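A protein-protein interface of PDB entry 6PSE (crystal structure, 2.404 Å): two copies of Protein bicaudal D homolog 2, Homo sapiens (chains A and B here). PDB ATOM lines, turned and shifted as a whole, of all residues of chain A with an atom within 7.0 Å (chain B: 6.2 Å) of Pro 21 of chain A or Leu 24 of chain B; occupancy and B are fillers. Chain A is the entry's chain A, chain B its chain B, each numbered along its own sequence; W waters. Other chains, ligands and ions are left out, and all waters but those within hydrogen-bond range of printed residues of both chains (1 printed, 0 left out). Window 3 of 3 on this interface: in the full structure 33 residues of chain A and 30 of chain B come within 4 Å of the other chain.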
ATOM      1  N   VAL A  16       5.802  10.677  -7.900  1.00  0.00           N
ATOM      2  CA  VAL A  16       6.404  11.848  -7.272  1.00  0.00           C
ATOM      3  C   VAL A  16       6.990  12.781  -8.321  1.00  0.00           C
ATOM      4  O   VAL A  16       6.773  14.001  -8.288  1.00  0.00           O
ATOM      5  CB  VAL A  16       7.450  11.406  -6.236  1.00  0.00           C
ATOM      6  CG1 VAL A  16       8.208  12.607  -5.676  1.00  0.00           C
ATOM      7  CG2 VAL A  16       6.741  10.655  -5.126  1.00  0.00           C
ATOM      8  N   ALA A  19       3.545  13.969 -10.637  1.00  0.00           N
ATOM      9  CA  ALA A  19       2.254  14.402 -10.105  1.00  0.00           C
ATOM     10  C   ALA A  19       2.183  15.934 -10.004  1.00  0.00           C
ATOM     11  O   ALA A  19       3.200  16.637 -10.055  1.00  0.00           O
ATOM     12  CB  ALA A  19       2.010  13.780  -8.719  1.00  0.00           C
ATOM     13  N   GLN A  20       0.954  16.452  -9.836  1.00  0.00           N
ATOM     14  CA  GLN A  20       0.739  17.891  -9.691  1.00  0.00           C
ATOM     15  C   GLN A  20       1.057  18.345  -8.268  1.00  0.00           C
ATOM     16  O   GLN A  20       1.117  17.529  -7.343  1.00  0.00           O
ATOM     17  CB  GLN A  20      -0.703  18.258 -10.042  1.00  0.00           C
ATOM     18  CG  GLN A  20      -0.991  18.410 -11.530  1.00  0.00           C
ATOM     19  CD  GLN A  20      -0.153  19.488 -12.184  1.00  0.00           C
ATOM     20  OE1 GLN A  20       0.728  19.196 -12.995  1.00  0.00           O
ATOM     21  NE2 GLN A  20      -0.419  20.740 -11.830  1.00  0.00           N
ATOM     22  N   PRO A  21       1.259  19.652  -8.063  1.00  0.00           N
ATOM     23  CA  PRO A  21       1.595  20.138  -6.707  1.00  0.00           C
ATOM     24  C   PRO A  21       0.548  19.827  -5.640  1.00  0.00           C
ATOM     25  O   PRO A  21       0.908  19.622  -4.471  1.00  0.00           O
ATOM     26  CB  PRO A  21       1.759  21.651  -6.916  1.00  0.00           C
ATOM     27  CG  PRO A  21       2.196  21.768  -8.352  1.00  0.00           C
ATOM     28  CD  PRO A  21       1.424  20.706  -9.086  1.00  0.00           C
ATOM     29  N   GLU A  22      -0.737  19.795  -6.001  1.00  0.00           N
ATOM     30  CA  GLU A  22      -1.771  19.472  -5.025  1.00  0.00           C
ATOM     31  C   GLU A  22      -1.560  18.072  -4.465  1.00  0.00           C
ATOM     32  O   GLU A  22      -1.670  17.857  -3.251  1.00  0.00           O
ATOM     33  CB  GLU A  22      -3.153  19.611  -5.665  1.00  0.00           C
ATOM     34  CG  GLU A  22      -3.334  20.903  -6.510  1.00  0.00           C
ATOM     35  CD  GLU A  22      -2.771  20.814  -7.950  1.00  0.00           C
ATOM     36  OE1 GLU A  22      -1.748  21.483  -8.250  1.00  0.00           O
ATOM     37  OE2 GLU A  22      -3.356  20.085  -8.785  1.00  0.00           O
ATOM     38  N   TRP A  23      -1.202  17.119  -5.331  1.00  0.00           N
ATOM     39  CA  TRP A  23      -0.864  15.771  -4.886  1.00  0.00           C
ATOM     40  C   TRP A  23       0.406  15.769  -4.048  1.00  0.00           C
ATOM     41  O   TRP A  23       0.449  15.151  -2.977  1.00  0.00           O
ATOM     42  CB  TRP A  23      -0.706  14.846  -6.089  1.00  0.00           C
ATOM     43  CG  TRP A  23      -0.543  13.393  -5.729  1.00  0.00           C
ATOM     44  CD1 TRP A  23      -1.529  12.453  -5.660  1.00  0.00           C
ATOM     45  CD2 TRP A  23       0.688  12.707  -5.427  1.00  0.00           C
ATOM     46  NE1 TRP A  23      -0.992  11.231  -5.329  1.00  0.00           N
ATOM     47  CE2 TRP A  23       0.364  11.362  -5.174  1.00  0.00           C
ATOM     48  CE3 TRP A  23       2.030  13.104  -5.337  1.00  0.00           C
ATOM     49  CZ2 TRP A  23       1.325  10.415  -4.829  1.00  0.00           C
ATOM     50  CZ3 TRP A  23       2.987  12.155  -5.013  1.00  0.00           C
ATOM     51  CH2 TRP A  23       2.626  10.826  -4.768  1.00  0.00           C
ATOM     52  N   LEU A  24       1.460  16.441  -4.520  1.00  0.00           N
ATOM     53  CA  LEU A  24       2.700  16.473  -3.746  1.00  0.00           C
ATOM     54  C   LEU A  24       2.483  17.051  -2.349  1.00  0.00           C
ATOM     55  O   LEU A  24       3.136  16.633  -1.378  1.00  0.00           O
ATOM     56  CB  LEU A  24       3.759  17.277  -4.495  1.00  0.00           C
ATOM     57  CG  LEU A  24       4.295  16.567  -5.737  1.00  0.00           C
ATOM     58  CD1 LEU A  24       5.105  17.533  -6.607  1.00  0.00           C
ATOM     59  CD2 LEU A  24       5.124  15.342  -5.380  1.00  0.00           C
ATOM     60  N   ARG A  25       1.572  18.013  -2.226  1.00  0.00           N
ATOM     61  CA  ARG A  25       1.349  18.656  -0.944  1.00  0.00           C
ATOM     62  C   ARG A  25       0.636  17.707   0.010  1.00  0.00           C
ATOM     63  O   ARG A  25       0.906  17.699   1.216  1.00  0.00           O
ATOM     64  CB  ARG A  25       0.550  19.938  -1.163  1.00  0.00           C
ATOM     65  CG  ARG A  25       0.410  20.808   0.073  1.00  0.00           C
ATOM     66  CD  ARG A  25      -0.088  22.200  -0.284  1.00  0.00           C
ATOM     67  NE  ARG A  25       0.795  22.865  -1.241  1.00  0.00           N
ATOM     68  CZ  ARG A  25       0.462  23.170  -2.496  1.00  0.00           C
ATOM     69  NH1 ARG A  25       1.346  23.783  -3.281  1.00  0.00           N
ATOM     70  NH2 ARG A  25      -0.750  22.868  -2.968  1.00  0.00           N
ATOM     71  N   ALA A  26      -0.258  16.884  -0.524  1.00  0.00           N
ATOM     72  CA  ALA A  26      -0.959  15.911   0.298  1.00  0.00           C
ATOM     73  C   ALA A  26      -0.027  14.784   0.750  1.00  0.00           C
ATOM     74  O   ALA A  26      -0.073  14.372   1.921  1.00  0.00           O
ATOM     75  CB  ALA A  26      -2.159  15.367  -0.467  1.00  0.00           C
ATOM     76  N   GLU A  27       0.837  14.282  -0.152  1.00  0.00           N
ATOM     77  CA  GLU A  27       1.853  13.307   0.254  1.00  0.00           C
ATOM     78  C   GLU A  27       2.770  13.863   1.344  1.00  0.00           C
ATOM     79  O   GLU A  27       3.098  13.162   2.306  1.00  0.00           O
ATOM     80  CB  GLU A  27       2.689  12.871  -0.945  1.00  0.00           C
ATOM     81  CG  GLU A  27       2.158  11.679  -1.620  1.00  0.00           C
ATOM     82  CD  GLU A  27       2.113  10.459  -0.726  1.00  0.00           C
ATOM     83  OE1 GLU A  27       3.183   9.875  -0.461  1.00  0.00           O
ATOM     84  OE2 GLU A  27       0.999  10.072  -0.311  1.00  0.00           O
ATOM     85  N   VAL A  28       3.246  15.101   1.178  1.00  0.00           N
ATOM     86  CA  VAL A  28       4.045  15.725   2.228  1.00  0.00           C
ATOM     87  C   VAL A  28       3.283  15.681   3.544  1.00  0.00           C
ATOM     88  O   VAL A  28       3.821  15.303   4.595  1.00  0.00           O
ATOM     89  CB  VAL A  28       4.404  17.170   1.839  1.00  0.00           C
ATOM     90  CG1 VAL A  28       4.856  17.930   3.061  1.00  0.00           C
ATOM     91  CG2 VAL A  28       5.476  17.184   0.791  1.00  0.00           C
ATOM     92  N   GLN B  20       7.662  25.720  -8.199  1.00  0.00           N
ATOM     93  CA  GLN B  20       8.274  25.063  -7.034  1.00  0.00           C
ATOM     94  C   GLN B  20       7.828  23.650  -6.616  1.00  0.00           C
ATOM     95  O   GLN B  20       7.848  23.325  -5.429  1.00  0.00           O
ATOM     96  CB  GLN B  20       8.114  25.952  -5.822  1.00  0.00           C
ATOM     97  CG  GLN B  20       6.777  25.817  -5.137  1.00  0.00           C
ATOM     98  CD  GLN B  20       6.866  26.222  -3.690  1.00  0.00           C
ATOM     99  OE1 GLN B  20       7.871  26.771  -3.257  1.00  0.00           O
ATOM    100  NE2 GLN B  20       5.819  25.953  -2.933  1.00  0.00           N
ATOM    101  N   PRO B  21       7.411  22.806  -7.543  1.00  0.00           N
ATOM    102  CA  PRO B  21       7.048  21.447  -7.122  1.00  0.00           C
ATOM    103  C   PRO B  21       8.367  20.751  -6.884  1.00  0.00           C
ATOM    104  O   PRO B  21       8.381  19.631  -6.354  1.00  0.00           O
ATOM    105  CB  PRO B  21       6.345  20.897  -8.370  1.00  0.00           C
ATOM    106  CG  PRO B  21       5.764  22.085  -9.069  1.00  0.00           C
ATOM    107  CD  PRO B  21       6.154  23.334  -8.342  1.00  0.00           C
ATOM    108  N   GLU B  22       9.485  21.366  -7.255  1.00  0.00           N
ATOM    109  CA  GLU B  22      10.748  20.720  -6.957  1.00  0.00           C
ATOM    110  C   GLU B  22      11.030  20.747  -5.457  1.00  0.00           C
ATOM    111  O   GLU B  22      11.725  19.866  -4.938  1.00  0.00           O
ATOM    112  CB  GLU B  22      11.874  21.366  -7.767  1.00  0.00           C
ATOM    113  CG  GLU B  22      13.278  20.820  -7.465  1.00  0.00           C
ATOM    114  CD  GLU B  22      13.328  19.296  -7.342  1.00  0.00           C
ATOM    115  OE1 GLU B  22      13.783  18.795  -6.282  1.00  0.00           O
ATOM    116  OE2 GLU B  22      12.899  18.604  -8.295  1.00  0.00           O
ATOM    117  N   TRP B  23      10.480  21.722  -4.731  1.00  0.00           N
ATOM    118  CA  TRP B  23      10.705  21.724  -3.289  1.00  0.00           C
ATOM    119  C   TRP B  23       9.835  20.671  -2.607  1.00  0.00           C
ATOM    120  O   TRP B  23      10.328  19.878  -1.801  1.00  0.00           O
ATOM    121  CB  TRP B  23      10.441  23.108  -2.692  1.00  0.00           C
ATOM    122  CG  TRP B  23      10.602  23.092  -1.195  1.00  0.00           C
ATOM    123  CD1 TRP B  23      11.775  23.137  -0.493  1.00  0.00           C
ATOM    124  CD2 TRP B  23       9.557  22.987  -0.222  1.00  0.00           C
ATOM    125  NE1 TRP B  23      11.525  23.087   0.854  1.00  0.00           N
ATOM    126  CE2 TRP B  23      10.172  22.991   1.051  1.00  0.00           C
ATOM    127  CE3 TRP B  23       8.161  22.890  -0.301  1.00  0.00           C
ATOM    128  CZ2 TRP B  23       9.441  22.907   2.238  1.00  0.00           C
ATOM    129  CZ3 TRP B  23       7.435  22.802   0.875  1.00  0.00           C
ATOM    130  CH2 TRP B  23       8.076  22.813   2.128  1.00  0.00           C
ATOM    131  N   LEU B  24       8.535  20.664  -2.922  1.00  0.00           N
ATOM    132  CA  LEU B  24       7.642  19.594  -2.497  1.00  0.00           C
ATOM    133  C   LEU B  24       8.257  18.223  -2.733  1.00  0.00           C
ATOM    134  O   LEU B  24       8.293  17.378  -1.824  1.00  0.00           O
ATOM    135  CB  LEU B  24       6.324  19.711  -3.252  1.00  0.00           C
ATOM    136  CG  LEU B  24       5.532  20.969  -2.939  1.00  0.00           C
ATOM    137  CD1 LEU B  24       4.272  20.953  -3.793  1.00  0.00           C
ATOM    138  CD2 LEU B  24       5.194  21.019  -1.449  1.00  0.00           C
ATOM    139  N   ARG B  25       8.719  17.976  -3.965  1.00  0.00           N
ATOM    140  CA  ARG B  25       9.329  16.694  -4.302  1.00  0.00           C
ATOM    141  C   ARG B  25      10.533  16.416  -3.425  1.00  0.00           C
ATOM    142  O   ARG B  25      10.782  15.263  -3.044  1.00  0.00           O
ATOM    143  CB  ARG B  25       9.752  16.679  -5.766  1.00  0.00           C
ATOM    144  CG  ARG B  25       8.644  16.379  -6.724  1.00  0.00           C
ATOM    145  CD  ARG B  25       9.194  16.194  -8.108  1.00  0.00           C
ATOM    146  NE  ARG B  25       8.514  17.081  -9.041  1.00  0.00           N
ATOM    147  CZ  ARG B  25       9.122  17.972  -9.809  1.00  0.00           C
ATOM    148  NH1 ARG B  25      10.449  18.096  -9.775  1.00  0.00           N
ATOM    149  NH2 ARG B  25       8.395  18.726 -10.618  1.00  0.00           N
ATOM    150  N   ALA B  26      11.305  17.459  -3.110  1.00  0.00           N
ATOM    151  CA  ALA B  26      12.405  17.298  -2.168  1.00  0.00           C
ATOM    152  C   ALA B  26      11.889  16.938  -0.775  1.00  0.00           C
ATOM    153  O   ALA B  26      12.505  16.131  -0.074  1.00  0.00           O
ATOM    154  CB  ALA B  26      13.249  18.571  -2.126  1.00  0.00           C
ATOM    155  N   GLU B  27      10.751  17.510  -0.373  1.00  0.00           N
ATOM    156  CA  GLU B  27      10.187  17.234   0.943  1.00  0.00           C
ATOM    157  C   GLU B  27       9.653  15.810   1.038  1.00  0.00           C
ATOM    158  O   GLU B  27       9.856  15.130   2.055  1.00  0.00           O
ATOM    159  CB  GLU B  27       9.077  18.233   1.238  1.00  0.00           C
ATOM    160  CG  GLU B  27       9.588  19.518   1.777  1.00  0.00           C
ATOM    161  CD  GLU B  27      10.405  19.310   3.027  1.00  0.00           C
ATOM    162  OE1 GLU B  27       9.803  19.114   4.110  1.00  0.00           O
ATOM    163  OE2 GLU B  27      11.652  19.346   2.922  1.00  0.00           O
ATOM    164  N   VAL B  28       8.946  15.353  -0.003  1.00  0.00           N
ATOM    165  CA  VAL B  28       8.469  13.973  -0.052  1.00  0.00           C
ATOM    166  C   VAL B  28       9.633  13.002   0.135  1.00  0.00           C
ATOM    167  O   VAL B  28       9.549  12.041   0.912  1.00  0.00           O
ATOM    168  CB  VAL B  28       7.724  13.702  -1.374  1.00  0.00           C
ATOM    169  CG1 VAL B  28       7.514  12.209  -1.579  1.00  0.00           C
ATOM    170  CG2 VAL B  28       6.387  14.453  -1.427  1.00  0.00           C
ATOM    171  N   LYS B  29      10.743  13.242  -0.565  1.00  0.00           N
ATOM    172  CA  LYS B  29      11.837  12.287  -0.446  1.00  0.00           C
ATOM    173  C   LYS B  29      12.536  12.396   0.901  1.00  0.00           C
ATOM    174  O   LYS B  29      12.968  11.378   1.458  1.00  0.00           O
ATOM    175  CB  LYS B  29      12.821  12.452  -1.597  1.00  0.00           C
ATOM    176  CG  LYS B  29      12.215  11.998  -2.913  1.00  0.00           C
ATOM    177  CD  LYS B  29      13.197  12.006  -4.061  1.00  0.00           C
ATOM    178  CE  LYS B  29      13.505  13.411  -4.503  1.00  0.00           C
ATOM    179  NZ  LYS B  29      13.019  13.664  -5.892  1.00  0.00           N
HETATM  180  O   HOH W   1       6.108  16.305  -9.642  1.00  0.00           O
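The side-chain carboxylate (OE2) of Glu 22 of chain B lies within salt-bridge range of the guanidinium group (NH1) of Arg 25 of chain B, 2.9 Å away.
Among the printed residues, pairs that only touch across the chains: Val 16 of chain A with Arg 25 of chain B (3.3 Å), Val 28 of chain A with Val 28 of chain B (3.6 Å), Pro 21 of chain A with Pro 21 of chain B (3.7 Å), Pro 21 of chain A with Leu 24 of chain B (3.7 Å), Leu 24 of chain A with Arg 25 of chain B (3.7 Å), Leu 24 of chain A with Leu 24 of chain B (3.7 Å), Val 28 of chain A with Glu 27 of chain B (3.8 Å), Val 28 of chain A with Leu 24 of chain B (3.8 Å), Leu 24 of chain A with Pro 21 of chain B (3.9 Å), Leu 24 of chain A with Val 28 of chain B (3.9 Å) and Val 16 of chain A with Val 28 of chain B (3.9 Å).
Pro 21 of chain A touches just these residues of chain B: Pro 21 and Leu 24.
Glu 22 of chain A touches none of the printed residues of chain B.
Leu 24 of chain B touches just these residues of chain A: Pro 21, Leu 24 and Val 28.
Of the printed residues of chain A, Arg 25 of chain B touches Val 16 (3.3 Å) and Leu 24 (3.7 Å).
Ala 26 of chain B touches none of the printed residues of chain A.
Printed residues of chain A within 4 Å of Glu 27 of chain B: Val 28 (3.8 Å).
The nearest residue of chain A that does not touch Leu 24 of chain B is Arg 25 of chain A (4.1 Å).
The nearest printed residue of chain B that does not touch Leu 24 of chain A is Glu 22 of chain B (5.9 Å).
Hydrophobic or aromatic side chains of chain B within 4 Å of the printed part of chain A: Pro 21, Leu 24 and Val 28.
Of the 11 printed residues of chain A, 4 touch a printed residue of chain B.
Hydrophobic or aromatic side chains of chain A within 4 Å of the printed part of chain B: Val 16, Pro 21, Leu 24 and Val 28.
Along chain A the printed residues that touch a printed residue of chain B span positions 16 to 28.
Among the printed residues, 11 pairs touch across the chains.
Pro 21 of chain A touches its own counterpart, Pro 21 of chain B.
Pro 21 of chain A touches Leu 24 of chain B, and with the chains exchanged Leu 24 of chain A touches Pro 21 of chain B.
Leu 24 of chain A touches Arg 25 of chain B, but with the chains exchanged Arg 25 of chain A does not touch Leu 24 of chain B (4.1 Å).
Val 28 of chain B touches its own counterpart, Val 28 of chain A.
Positions printed for both chains: 20, 21, 22, 23, 24, 25, 26, 27 and 28.
Of the 11 pairs that touch across the chains among the printed residues, 7 have their exchanged pair printed and touching as well.
Water W1 lies within hydrogen-bond range of NE of Arg 25 of chain B (2.6 Å), O of Val 16 of chain A (2.8 Å) and O of Ala 19 of chain A (3.0 Å).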
